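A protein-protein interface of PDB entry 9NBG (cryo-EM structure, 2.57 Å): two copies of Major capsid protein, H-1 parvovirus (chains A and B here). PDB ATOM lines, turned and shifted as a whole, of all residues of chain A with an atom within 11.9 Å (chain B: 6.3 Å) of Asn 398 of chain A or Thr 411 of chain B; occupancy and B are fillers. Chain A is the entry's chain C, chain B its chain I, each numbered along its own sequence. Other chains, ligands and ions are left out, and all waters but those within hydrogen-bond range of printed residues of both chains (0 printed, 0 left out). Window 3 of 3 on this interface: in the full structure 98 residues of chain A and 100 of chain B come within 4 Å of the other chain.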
ATOM      1  N   PHE A 385      15.933   1.742  32.516  1.00  0.00           N
ATOM      2  CA  PHE A 385      15.377   2.792  31.626  1.00  0.00           C
ATOM      3  C   PHE A 385      16.401   3.918  31.457  1.00  0.00           C
ATOM      4  O   PHE A 385      17.231   4.118  32.364  1.00  0.00           O
ATOM      5  CB  PHE A 385      14.057   3.339  32.173  1.00  0.00           C
ATOM      6  CG  PHE A 385      14.157   4.045  33.501  1.00  0.00           C
ATOM      7  CD1 PHE A 385      13.948   5.412  33.594  1.00  0.00           C
ATOM      8  CD2 PHE A 385      14.431   3.345  34.664  1.00  0.00           C
ATOM      9  CE1 PHE A 385      14.035   6.064  34.813  1.00  0.00           C
ATOM     10  CE2 PHE A 385      14.515   3.996  35.883  1.00  0.00           C
ATOM     11  CZ  PHE A 385      14.317   5.354  35.956  1.00  0.00           C
ATOM     12  N   VAL A 386      16.341   4.624  30.327  1.00  0.00           N
ATOM     13  CA  VAL A 386      17.265   5.771  30.082  1.00  0.00           C
ATOM     14  C   VAL A 386      16.413   7.008  29.791  1.00  0.00           C
ATOM     15  O   VAL A 386      15.449   6.886  29.014  1.00  0.00           O
ATOM     16  CB  VAL A 386      18.236   5.472  28.925  1.00  0.00           C
ATOM     17  CG1 VAL A 386      19.173   6.639  28.658  1.00  0.00           C
ATOM     18  CG2 VAL A 386      19.024   4.193  29.162  1.00  0.00           C
ATOM     19  N   GLN A 387      16.703   8.135  30.444  1.00  0.00           N
ATOM     20  CA  GLN A 387      15.864   9.350  30.261  1.00  0.00           C
ATOM     21  C   GLN A 387      16.681  10.428  29.548  1.00  0.00           C
ATOM     22  O   GLN A 387      17.911  10.263  29.448  1.00  0.00           O
ATOM     23  CB  GLN A 387      15.323   9.852  31.599  1.00  0.00           C
ATOM     24  CG  GLN A 387      14.286   8.926  32.218  1.00  0.00           C
ATOM     25  CD  GLN A 387      13.441   9.636  33.246  1.00  0.00           C
ATOM     26  OE1 GLN A 387      13.581  10.836  33.475  1.00  0.00           O
ATOM     27  NE2 GLN A 387      12.538   8.896  33.870  1.00  0.00           N
ATOM     28  N   SER A 388      16.021  11.490  29.081  1.00  0.00           N
ATOM     29  CA  SER A 388      16.726  12.544  28.308  1.00  0.00           C
ATOM     30  C   SER A 388      17.062  13.734  29.207  1.00  0.00           C
ATOM     31  O   SER A 388      16.166  14.184  29.941  1.00  0.00           O
ATOM     32  CB  SER A 388      15.889  12.979  27.137  1.00  0.00           C
ATOM     33  OG  SER A 388      14.653  13.515  27.580  1.00  0.00           O
ATOM     34  N   ALA A 389      18.287  14.255  29.106  1.00  0.00           N
ATOM     35  CA  ALA A 389      18.681  15.451  29.886  1.00  0.00           C
ATOM     36  C   ALA A 389      18.447  16.706  29.038  1.00  0.00           C
ATOM     37  O   ALA A 389      18.869  16.705  27.868  1.00  0.00           O
ATOM     38  CB  ALA A 389      20.120  15.333  30.308  1.00  0.00           C
ATOM     39  N   PRO A 390      17.795  17.770  29.556  1.00  0.00           N
ATOM     40  CA  PRO A 390      17.603  17.954  31.000  1.00  0.00           C
ATOM     41  C   PRO A 390      16.529  17.002  31.546  1.00  0.00           C
ATOM     42  O   PRO A 390      15.457  16.941  30.974  1.00  0.00           O
ATOM     43  CB  PRO A 390      17.151  19.416  31.109  1.00  0.00           C
ATOM     44  CG  PRO A 390      16.462  19.693  29.794  1.00  0.00           C
ATOM     45  CD  PRO A 390      17.216  18.865  28.775  1.00  0.00           C
ATOM     46  N   ILE A 391      16.842  16.289  32.629  1.00  0.00           N
ATOM     47  CA  ILE A 391      15.893  15.262  33.163  1.00  0.00           C
ATOM     48  C   ILE A 391      14.515  15.885  33.402  1.00  0.00           C
ATOM     49  O   ILE A 391      14.441  16.931  34.072  1.00  0.00           O
ATOM     50  CB  ILE A 391      16.466  14.599  34.433  1.00  0.00           C
ATOM     51  CG1 ILE A 391      15.557  13.482  34.952  1.00  0.00           C
ATOM     52  CG2 ILE A 391      16.767  15.633  35.509  1.00  0.00           C
ATOM     53  CD1 ILE A 391      16.170  12.664  36.061  1.00  0.00           C
ATOM     54  N   SER A 392      13.468  15.271  32.850  1.00  0.00           N
ATOM     55  CA  SER A 392      12.084  15.745  33.093  1.00  0.00           C
ATOM     56  C   SER A 392      11.289  14.618  33.752  1.00  0.00           C
ATOM     57  O   SER A 392      10.892  13.688  33.034  1.00  0.00           O
ATOM     58  CB  SER A 392      11.437  16.190  31.815  1.00  0.00           C
ATOM     59  OG  SER A 392      12.219  17.189  31.176  1.00  0.00           O
ATOM     60  N   ILE A 393      11.020  14.737  35.056  1.00  0.00           N
ATOM     61  CA  ILE A 393      10.179  13.736  35.771  1.00  0.00           C
ATOM     62  C   ILE A 393       8.834  14.400  36.080  1.00  0.00           C
ATOM     63  O   ILE A 393       8.851  15.532  36.592  1.00  0.00           O
ATOM     64  CB  ILE A 393      10.880  13.266  37.059  1.00  0.00           C
ATOM     65  CG1 ILE A 393      12.355  12.942  36.815  1.00  0.00           C
ATOM     66  CG2 ILE A 393      10.139  12.096  37.684  1.00  0.00           C
ATOM     67  CD1 ILE A 393      13.106  12.542  38.065  1.00  0.00           C
ATOM     68  N   PRO A 394       7.672  13.768  35.795  1.00  0.00           N
ATOM     69  CA  PRO A 394       7.616  12.557  34.978  1.00  0.00           C
ATOM     70  C   PRO A 394       7.891  12.843  33.496  1.00  0.00           C
ATOM     71  O   PRO A 394       7.507  13.890  33.015  1.00  0.00           O
ATOM     72  CB  PRO A 394       6.164  12.090  35.139  1.00  0.00           C
ATOM     73  CG  PRO A 394       5.398  13.358  35.426  1.00  0.00           C
ATOM     74  CD  PRO A 394       6.350  14.198  36.252  1.00  0.00           C
ATOM     75  N   PRO A 395       8.552  11.924  32.742  1.00  0.00           N
ATOM     76  CA  PRO A 395       8.851  12.155  31.331  1.00  0.00           C
ATOM     77  C   PRO A 395       7.690  11.773  30.402  1.00  0.00           C
ATOM     78  O   PRO A 395       6.734  11.189  30.875  1.00  0.00           O
ATOM     79  CB  PRO A 395      10.024  11.199  31.073  1.00  0.00           C
ATOM     80  CG  PRO A 395       9.716  10.014  31.948  1.00  0.00           C
ATOM     81  CD  PRO A 395       9.074  10.617  33.181  1.00  0.00           C
ATOM     82  N   ASN A 396       7.804  12.114  29.117  1.00  0.00           N
ATOM     83  CA  ASN A 396       6.753  11.736  28.133  1.00  0.00           C
ATOM     84  C   ASN A 396       7.285  10.598  27.254  1.00  0.00           C
ATOM     85  O   ASN A 396       8.494  10.312  27.330  1.00  0.00           O
ATOM     86  CB  ASN A 396       6.276  12.930  27.305  1.00  0.00           C
ATOM     87  CG  ASN A 396       7.399  13.677  26.619  1.00  0.00           C
ATOM     88  OD1 ASN A 396       8.142  13.103  25.825  1.00  0.00           O
ATOM     89  ND2 ASN A 396       7.523  14.960  26.911  1.00  0.00           N
ATOM     90  N   GLN A 397       6.419   9.992  26.442  1.00  0.00           N
ATOM     91  CA  GLN A 397       6.837   8.842  25.597  1.00  0.00           C
ATOM     92  C   GLN A 397       8.122   9.185  24.839  1.00  0.00           C
ATOM     93  O   GLN A 397       8.828   8.245  24.438  1.00  0.00           O
ATOM     94  CB  GLN A 397       5.725   8.482  24.611  1.00  0.00           C
ATOM     95  CG  GLN A 397       5.249   9.664  23.781  1.00  0.00           C
ATOM     96  CD  GLN A 397       4.276   9.245  22.708  1.00  0.00           C
ATOM     97  OE1 GLN A 397       3.940   8.070  22.573  1.00  0.00           O
ATOM     98  NE2 GLN A 397       3.815  10.210  21.931  1.00  0.00           N
ATOM     99  N   ASN A 398       8.415  10.474  24.648  1.00  0.00           N
ATOM    100  CA  ASN A 398       9.591  10.861  23.825  1.00  0.00           C
ATOM    101  C   ASN A 398      10.744  11.331  24.717  1.00  0.00           C
ATOM    102  O   ASN A 398      11.744  11.825  24.164  1.00  0.00           O
ATOM    103  CB  ASN A 398       9.225  11.927  22.791  1.00  0.00           C
ATOM    104  CG  ASN A 398       8.229  11.434  21.762  1.00  0.00           C
ATOM    105  OD1 ASN A 398       7.825  10.274  21.788  1.00  0.00           O
ATOM    106  ND2 ASN A 398       7.834  12.306  20.851  1.00  0.00           N
ATOM    107  N   GLN A 399      10.618  11.166  26.035  1.00  0.00           N
ATOM    108  CA  GLN A 399      11.669  11.662  26.963  1.00  0.00           C
ATOM    109  C   GLN A 399      12.279  10.487  27.735  1.00  0.00           C
ATOM    110  O   GLN A 399      13.117  10.742  28.621  1.00  0.00           O
ATOM    111  CB  GLN A 399      11.083  12.698  27.922  1.00  0.00           C
ATOM    112  CG  GLN A 399      11.071  14.110  27.357  1.00  0.00           C
ATOM    113  CD  GLN A 399      10.349  15.068  28.271  1.00  0.00           C
ATOM    114  OE1 GLN A 399       9.787  14.677  29.289  1.00  0.00           O
ATOM    115  NE2 GLN A 399      10.344  16.337  27.898  1.00  0.00           N
ATOM    116  N   ILE A 400      11.876   9.257  27.405  1.00  0.00           N
ATOM    117  CA  ILE A 400      12.396   8.061  28.132  1.00  0.00           C
ATOM    118  C   ILE A 400      12.621   6.915  27.140  1.00  0.00           C
ATOM    119  O   ILE A 400      11.805   6.766  26.212  1.00  0.00           O
ATOM    120  CB  ILE A 400      11.442   7.649  29.272  1.00  0.00           C
ATOM    121  CG1 ILE A 400      11.972   6.440  30.045  1.00  0.00           C
ATOM    122  CG2 ILE A 400      10.035   7.410  28.747  1.00  0.00           C
ATOM    123  CD1 ILE A 400      11.093   6.012  31.193  1.00  0.00           C
ATOM    124  N   LEU A 401      13.689   6.140  27.330  1.00  0.00           N
ATOM    125  CA  LEU A 401      13.929   4.960  26.460  1.00  0.00           C
ATOM    126  C   LEU A 401      13.602   3.703  27.268  1.00  0.00           C
ATOM    127  O   LEU A 401      14.514   3.167  27.919  1.00  0.00           O
ATOM    128  CB  LEU A 401      15.389   4.969  26.001  1.00  0.00           C
ATOM    129  CG  LEU A 401      15.726   3.996  24.873  1.00  0.00           C
ATOM    130  CD1 LEU A 401      14.889   4.290  23.641  1.00  0.00           C
ATOM    131  CD2 LEU A 401      17.208   4.065  24.535  1.00  0.00           C
ATOM    132  N   GLN A 402      12.335   3.282  27.247  1.00  0.00           N
ATOM    133  CA  GLN A 402      11.926   2.046  27.960  1.00  0.00           C
ATOM    134  C   GLN A 402      12.413   0.847  27.146  1.00  0.00           C
ATOM    135  O   GLN A 402      12.767   1.033  25.969  1.00  0.00           O
ATOM    136  CB  GLN A 402      10.408   1.993  28.115  1.00  0.00           C
ATOM    137  CG  GLN A 402       9.805   3.278  28.661  1.00  0.00           C
ATOM    138  CD  GLN A 402       8.300   3.207  28.719  1.00  0.00           C
ATOM    139  OE1 GLN A 402       7.630   4.154  29.126  1.00  0.00           O
ATOM    140  NE2 GLN A 402       7.753   2.076  28.306  1.00  0.00           N
ATOM    141  N   GLU A 404      10.730  -1.862  26.023  1.00  0.00           N
ATOM    142  CA  GLU A 404       9.823  -2.274  24.916  1.00  0.00           C
ATOM    143  C   GLU A 404      10.136  -1.490  23.635  1.00  0.00           C
ATOM    144  O   GLU A 404       9.736  -1.959  22.555  1.00  0.00           O
ATOM    145  CB  GLU A 404       8.361  -2.104  25.334  1.00  0.00           C
ATOM    146  CG  GLU A 404       7.908  -0.661  25.415  1.00  0.00           C
ATOM    147  CD  GLU A 404       6.433  -0.511  25.746  1.00  0.00           C
ATOM    148  OE1 GLU A 404       5.764  -1.544  25.946  1.00  0.00           O
ATOM    149  OE2 GLU A 404       5.952   0.639  25.794  1.00  0.00           O
ATOM    150  N   ASP A 405      10.799  -0.339  23.759  1.00  0.00           N
ATOM    151  CA  ASP A 405      11.093   0.504  22.570  1.00  0.00           C
ATOM    152  C   ASP A 405      11.894  -0.321  21.557  1.00  0.00           C
ATOM    153  O   ASP A 405      12.979  -0.810  21.921  1.00  0.00           O
ATOM    154  CB  ASP A 405      11.806   1.796  22.974  1.00  0.00           C
ATOM    155  CG  ASP A 405      10.900   2.764  23.712  1.00  0.00           C
ATOM    156  OD1 ASP A 405       9.694   2.470  23.815  1.00  0.00           O
ATOM    157  OD2 ASP A 405      11.411   3.796  24.193  1.00  0.00           O
ATOM    158  N   ALA A 406      11.371  -0.463  20.337  1.00  0.00           N
ATOM    159  CA  ALA A 406      12.057  -1.260  19.292  1.00  0.00           C
ATOM    160  C   ALA A 406      13.265  -0.489  18.757  1.00  0.00           C
ATOM    161  O   ALA A 406      13.188   0.750  18.676  1.00  0.00           O
ATOM    162  CB  ALA A 406      11.088  -1.588  18.184  1.00  0.00           C
ATOM    163  N   ILE A 407      14.332  -1.205  18.387  1.00  0.00           N
ATOM    164  CA  ILE A 407      15.547  -0.550  17.820  1.00  0.00           C
ATOM    165  C   ILE A 407      15.665  -0.944  16.345  1.00  0.00           C
ATOM    166  O   ILE A 407      15.473  -2.136  16.043  1.00  0.00           O
ATOM    167  CB  ILE A 407      16.803  -0.949  18.618  1.00  0.00           C
ATOM    168  CG1 ILE A 407      16.676  -0.559  20.092  1.00  0.00           C
ATOM    169  CG2 ILE A 407      18.055  -0.360  17.988  1.00  0.00           C
ATOM    170  CD1 ILE A 407      16.483   0.920  20.322  1.00  0.00           C
ATOM    171  N   ASN B 197       2.735   9.207  29.204  1.00  0.00           N
ATOM    172  CA  ASN B 197       1.873   8.987  28.013  1.00  0.00           C
ATOM    173  C   ASN B 197       1.426   7.523  27.951  1.00  0.00           C
ATOM    174  O   ASN B 197       0.786   7.148  26.952  1.00  0.00           O
ATOM    175  CB  ASN B 197       2.582   9.405  26.724  1.00  0.00           C
ATOM    176  CG  ASN B 197       3.004  10.858  26.728  1.00  0.00           C
ATOM    177  OD1 ASN B 197       2.753  11.580  27.690  1.00  0.00           O
ATOM    178  ND2 ASN B 197       3.642  11.298  25.657  1.00  0.00           N
ATOM    179  N   GLU B 404      20.725  15.244  16.964  1.00  0.00           N
ATOM    180  CA  GLU B 404      19.260  15.451  16.796  1.00  0.00           C
ATOM    181  C   GLU B 404      18.580  14.164  16.313  1.00  0.00           C
ATOM    182  O   GLU B 404      17.351  14.060  16.475  1.00  0.00           O
ATOM    183  CB  GLU B 404      18.993  16.618  15.843  1.00  0.00           C
ATOM    184  CG  GLU B 404      19.303  16.311  14.393  1.00  0.00           C
ATOM    185  CD  GLU B 404      18.951  17.447  13.448  1.00  0.00           C
ATOM    186  OE1 GLU B 404      18.490  18.498  13.935  1.00  0.00           O
ATOM    187  OE2 GLU B 404      19.128  17.276  12.225  1.00  0.00           O
ATOM    188  N   ASP B 405      19.345  13.241  15.727  1.00  0.00           N
ATOM    189  CA  ASP B 405      18.751  11.990  15.185  1.00  0.00           C
ATOM    190  C   ASP B 405      18.017  11.255  16.311  1.00  0.00           C
ATOM    191  O   ASP B 405      18.663  10.930  17.323  1.00  0.00           O
ATOM    192  CB  ASP B 405      19.815  11.122  14.511  1.00  0.00           C
ATOM    193  CG  ASP B 405      20.317  11.712  13.205  1.00  0.00           C
ATOM    194  OD1 ASP B 405      19.759  12.741  12.778  1.00  0.00           O
ATOM    195  OD2 ASP B 405      21.272  11.147  12.635  1.00  0.00           O
ATOM    196  N   ALA B 406      16.716  11.009  16.133  1.00  0.00           N
ATOM    197  CA  ALA B 406      15.911  10.324  17.171  1.00  0.00           C
ATOM    198  C   ALA B 406      16.257   8.834  17.202  1.00  0.00           C
ATOM    199  O   ALA B 406      16.540   8.270  16.129  1.00  0.00           O
ATOM    200  CB  ALA B 406      14.443  10.535  16.900  1.00  0.00           C
ATOM    201  N   ILE B 407      16.215   8.220  18.389  1.00  0.00           N
ATOM    202  CA  ILE B 407      16.501   6.762  18.518  1.00  0.00           C
ATOM    203  C   ILE B 407      15.204   6.046  18.905  1.00  0.00           C
ATOM    204  O   ILE B 407      14.494   6.563  19.786  1.00  0.00           O
ATOM    205  CB  ILE B 407      17.616   6.516  19.553  1.00  0.00           C
ATOM    206  CG1 ILE B 407      18.908   7.238  19.165  1.00  0.00           C
ATOM    207  CG2 ILE B 407      17.847   5.027  19.758  1.00  0.00           C
ATOM    208  CD1 ILE B 407      19.470   6.817  17.830  1.00  0.00           C
ATOM    209  N   GLY B 409      12.496   6.033  17.533  1.00  0.00           N
ATOM    210  CA  GLY B 409      11.319   6.885  17.282  1.00  0.00           C
ATOM    211  C   GLY B 409      11.048   7.837  18.432  1.00  0.00           C
ATOM    212  O   GLY B 409      10.098   8.633  18.321  1.00  0.00           O
ATOM    213  N   ARG B 410      11.851   7.770  19.495  1.00  0.00           N
ATOM    214  CA  ARG B 410      11.690   8.738  20.613  1.00  0.00           C
ATOM    215  C   ARG B 410      12.351  10.056  20.202  1.00  0.00           C
ATOM    216  O   ARG B 410      13.584  10.063  20.041  1.00  0.00           O
ATOM    217  CB  ARG B 410      12.264   8.150  21.904  1.00  0.00           C
ATOM    218  CG  ARG B 410      11.674   6.794  22.265  1.00  0.00           C
ATOM    219  CD  ARG B 410      10.159   6.843  22.216  1.00  0.00           C
ATOM    220  NE  ARG B 410       9.550   5.525  22.324  1.00  0.00           N
ATOM    221  CZ  ARG B 410       8.242   5.301  22.285  1.00  0.00           C
ATOM    222  NH1 ARG B 410       7.406   6.305  22.098  1.00  0.00           N
ATOM    223  NH2 ARG B 410       7.775   4.074  22.434  1.00  0.00           N
ATOM    224  N   THR B 411      11.565  11.123  20.053  1.00  0.00           N
ATOM    225  CA  THR B 411      12.104  12.414  19.546  1.00  0.00           C
ATOM    226  C   THR B 411      13.262  12.922  20.410  1.00  0.00           C
ATOM    227  O   THR B 411      14.292  13.308  19.826  1.00  0.00           O
ATOM    228  CB  THR B 411      10.994  13.468  19.484  1.00  0.00           C
ATOM    229  OG1 THR B 411       9.959  12.961  18.641  1.00  0.00           O
ATOM    230  CG2 THR B 411      11.475  14.803  18.957  1.00  0.00           C
ATOM    231  N   ASN B 412      13.112  12.917  21.733  1.00  0.00           N
ATOM    232  CA  ASN B 412      14.163  13.514  22.603  1.00  0.00           C
ATOM    233  C   ASN B 412      15.227  12.470  22.963  1.00  0.00           C
ATOM    234  O   ASN B 412      16.150  12.820  23.722  1.00  0.00           O
ATOM    235  CB  ASN B 412      13.556  14.157  23.853  1.00  0.00           C
ATOM    236  CG  ASN B 412      12.600  15.281  23.523  1.00  0.00           C
ATOM    237  OD1 ASN B 412      12.379  15.592  22.353  1.00  0.00           O
ATOM    238  ND2 ASN B 412      12.029  15.899  24.543  1.00  0.00           N
ATOM    239  N   MET B 413      15.121  11.248  22.444  1.00  0.00           N
ATOM    240  CA  MET B 413      16.184  10.245  22.720  1.00  0.00           C
ATOM    241  C   MET B 413      17.244  10.302  21.618  1.00  0.00           C
ATOM    242  O   MET B 413      16.866  10.245  20.435  1.00  0.00           O
ATOM    243  CB  MET B 413      15.609   8.830  22.810  1.00  0.00           C
ATOM    244  CG  MET B 413      15.023   8.507  24.172  1.00  0.00           C
ATOM    245  SD  MET B 413      16.112   8.964  25.542  1.00  0.00           S
ATOM    246  CE  MET B 413      15.278  10.423  26.163  1.00  0.00           C
ATOM    247  N   HIS B 414      18.519  10.408  22.000  1.00  0.00           N
ATOM    248  CA  HIS B 414      19.620  10.521  21.006  1.00  0.00           C
ATOM    249  C   HIS B 414      20.703   9.491  21.340  1.00  0.00           C
ATOM    250  O   HIS B 414      20.863   9.144  22.526  1.00  0.00           O
ATOM    251  CB  HIS B 414      20.164  11.951  20.992  1.00  0.00           C
ATOM    252  CG  HIS B 414      19.095  12.986  20.910  1.00  0.00           C
ATOM    253  ND1 HIS B 414      18.181  13.037  19.881  1.00  0.00           N
ATOM    254  CD2 HIS B 414      18.784  13.999  21.728  1.00  0.00           C
ATOM    255  CE1 HIS B 414      17.356  14.054  20.077  1.00  0.00           C
ATOM    256  NE2 HIS B 414      17.703  14.653  21.195  1.00  0.00           N
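Of the 22 printed residues of chain A, 9 touch a printed residue of chain B. Printed residues of chain A that touch a printed residue of chain B: Gln 387, Ser 388, Asn 396, Gln 397, Asn 398, Gln 399, Ile 400, Leu 401 and Asp 405. Hydrophobic or aromatic side chains of chain A within 4 Å of the printed part of chain B: Leu 401. Of the 11 printed residues of chain B, 5 touch a printed residue of chain A. Along chain B the printed residues that touch a printed residue of chain A span positions 197 to 413.
The backbone NH (N) of Gln 397 of chain A sits close to the side-chain amide nitrogen (ND2) of Asn 197 of chain B (3.2 Å). ND2 of Asn 398 of chain A is in hydrogen-bond range of OG1 of Thr 411 of chain B. The backbone carbonyl oxygen (O) of Asn 398 of chain A sits close to the backbone NH (N) of Asn 412 of chain B, 3.0 Å away. NH2 of Arg 410 of chain B is in salt-bridge range of OD1 of Asp 405 of chain A, at 2.9 Å. The guanidinium group (NH1) of Arg 410 of chain B sits close to the backbone carbonyl oxygen (O) of Gln 397 of chain A, 3.4 Å away.
Of the printed residues of chain B, Asn 398 of chain A touches Thr 411, Asn 412 and Met 413. Thr 411 of chain B touches just one residue of chain A: Asn 398. No residue of chain A comes within 4 Å of Gly 409 of chain B. Of chain A, only Ser 388, Asn 398 and Gln 399 come within 4 Å of Asn 412 of chain B. Printed residues of chain A within 4 Å of Asn 197 of chain B: Asn 396 (3.5 Å) and Gln 397 (3.0 Å). Printed residues of chain B within 4 Å of Gln 399 of chain A: Asn 412 and Met 413. Of the printed residues of chain B, Gln 387 of chain A touches Met 413. Printed residues of chain B within 4 Å of Ile 400 of chain A: Arg 410 (3.9 Å) and Met 413 (3.8 Å). Printed residues of chain B within 4 Å of Leu 401 of chain A: Met 413. Ile 393 of chain A touches none of the printed residues of chain B. The nearest printed residue of chain B that does not touch Asn 398 of chain A is Arg 410 of chain B (4.003 Å). The nearest residue of chain A that does not touch Thr 411 of chain B is Gln 397 of chain A (5.9 Å). The nearest printed residue of chain B that does not touch Ile 400 of chain A is Asn 412 of chain B (6.3 Å).
Positions printed for both chains: 404, 405, 406 and 407. Of the 15 pairs that touch across the chains among the printed residues, none has its exchanged pair printed and touching as well.
N of Gln 402 of chain A sits at hydrogen-bond distance from OD2 of Asp 405 of chain A, at 3.2 Å. The backbone NH of Ile 407 of chain B sits at hydrogen-bond distance from the backbone carbonyl oxygen of Met 413 of chain B. The backbone NH (N) of Ser 388 of chain A is in hydrogen-bond range of the backbone carbonyl oxygen (O) of Gln 399 of chain A, 3.0 Å away. The side-chain amide oxygen (OD1) of Asn 396 of chain A is in hydrogen-bond range of the backbone NH (N) of Gln 399 of chain A (3.2 Å). OD1 of Asn 396 of chain A lies close to N of Asn 398 of chain A, 2.9 Å away. O of Asn 412 of chain B sits at hydrogen-bond distance from NE2 of His 414 of chain B (3.5 Å).
Among the printed residues, merely in contact across the chains: Ser 388 of chain A with Met 413 of chain B, Gln 399 of chain A with Met 413 of chain B, Ser 388 of chain A with Asn 412 of chain B, Gln 399 of chain A with Asn 412 of chain B, Asn 396 of chain A with Asn 197 of chain B, Gln 387 of chain A with Met 413 of chain B, Ile 400 of chain A with Met 413 of chain B, Asn 398 of chain A with Met 413 of chain B, Ile 400 of chain A with Arg 410 of chain B and Leu 401 of chain A with Met 413 of chain B.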
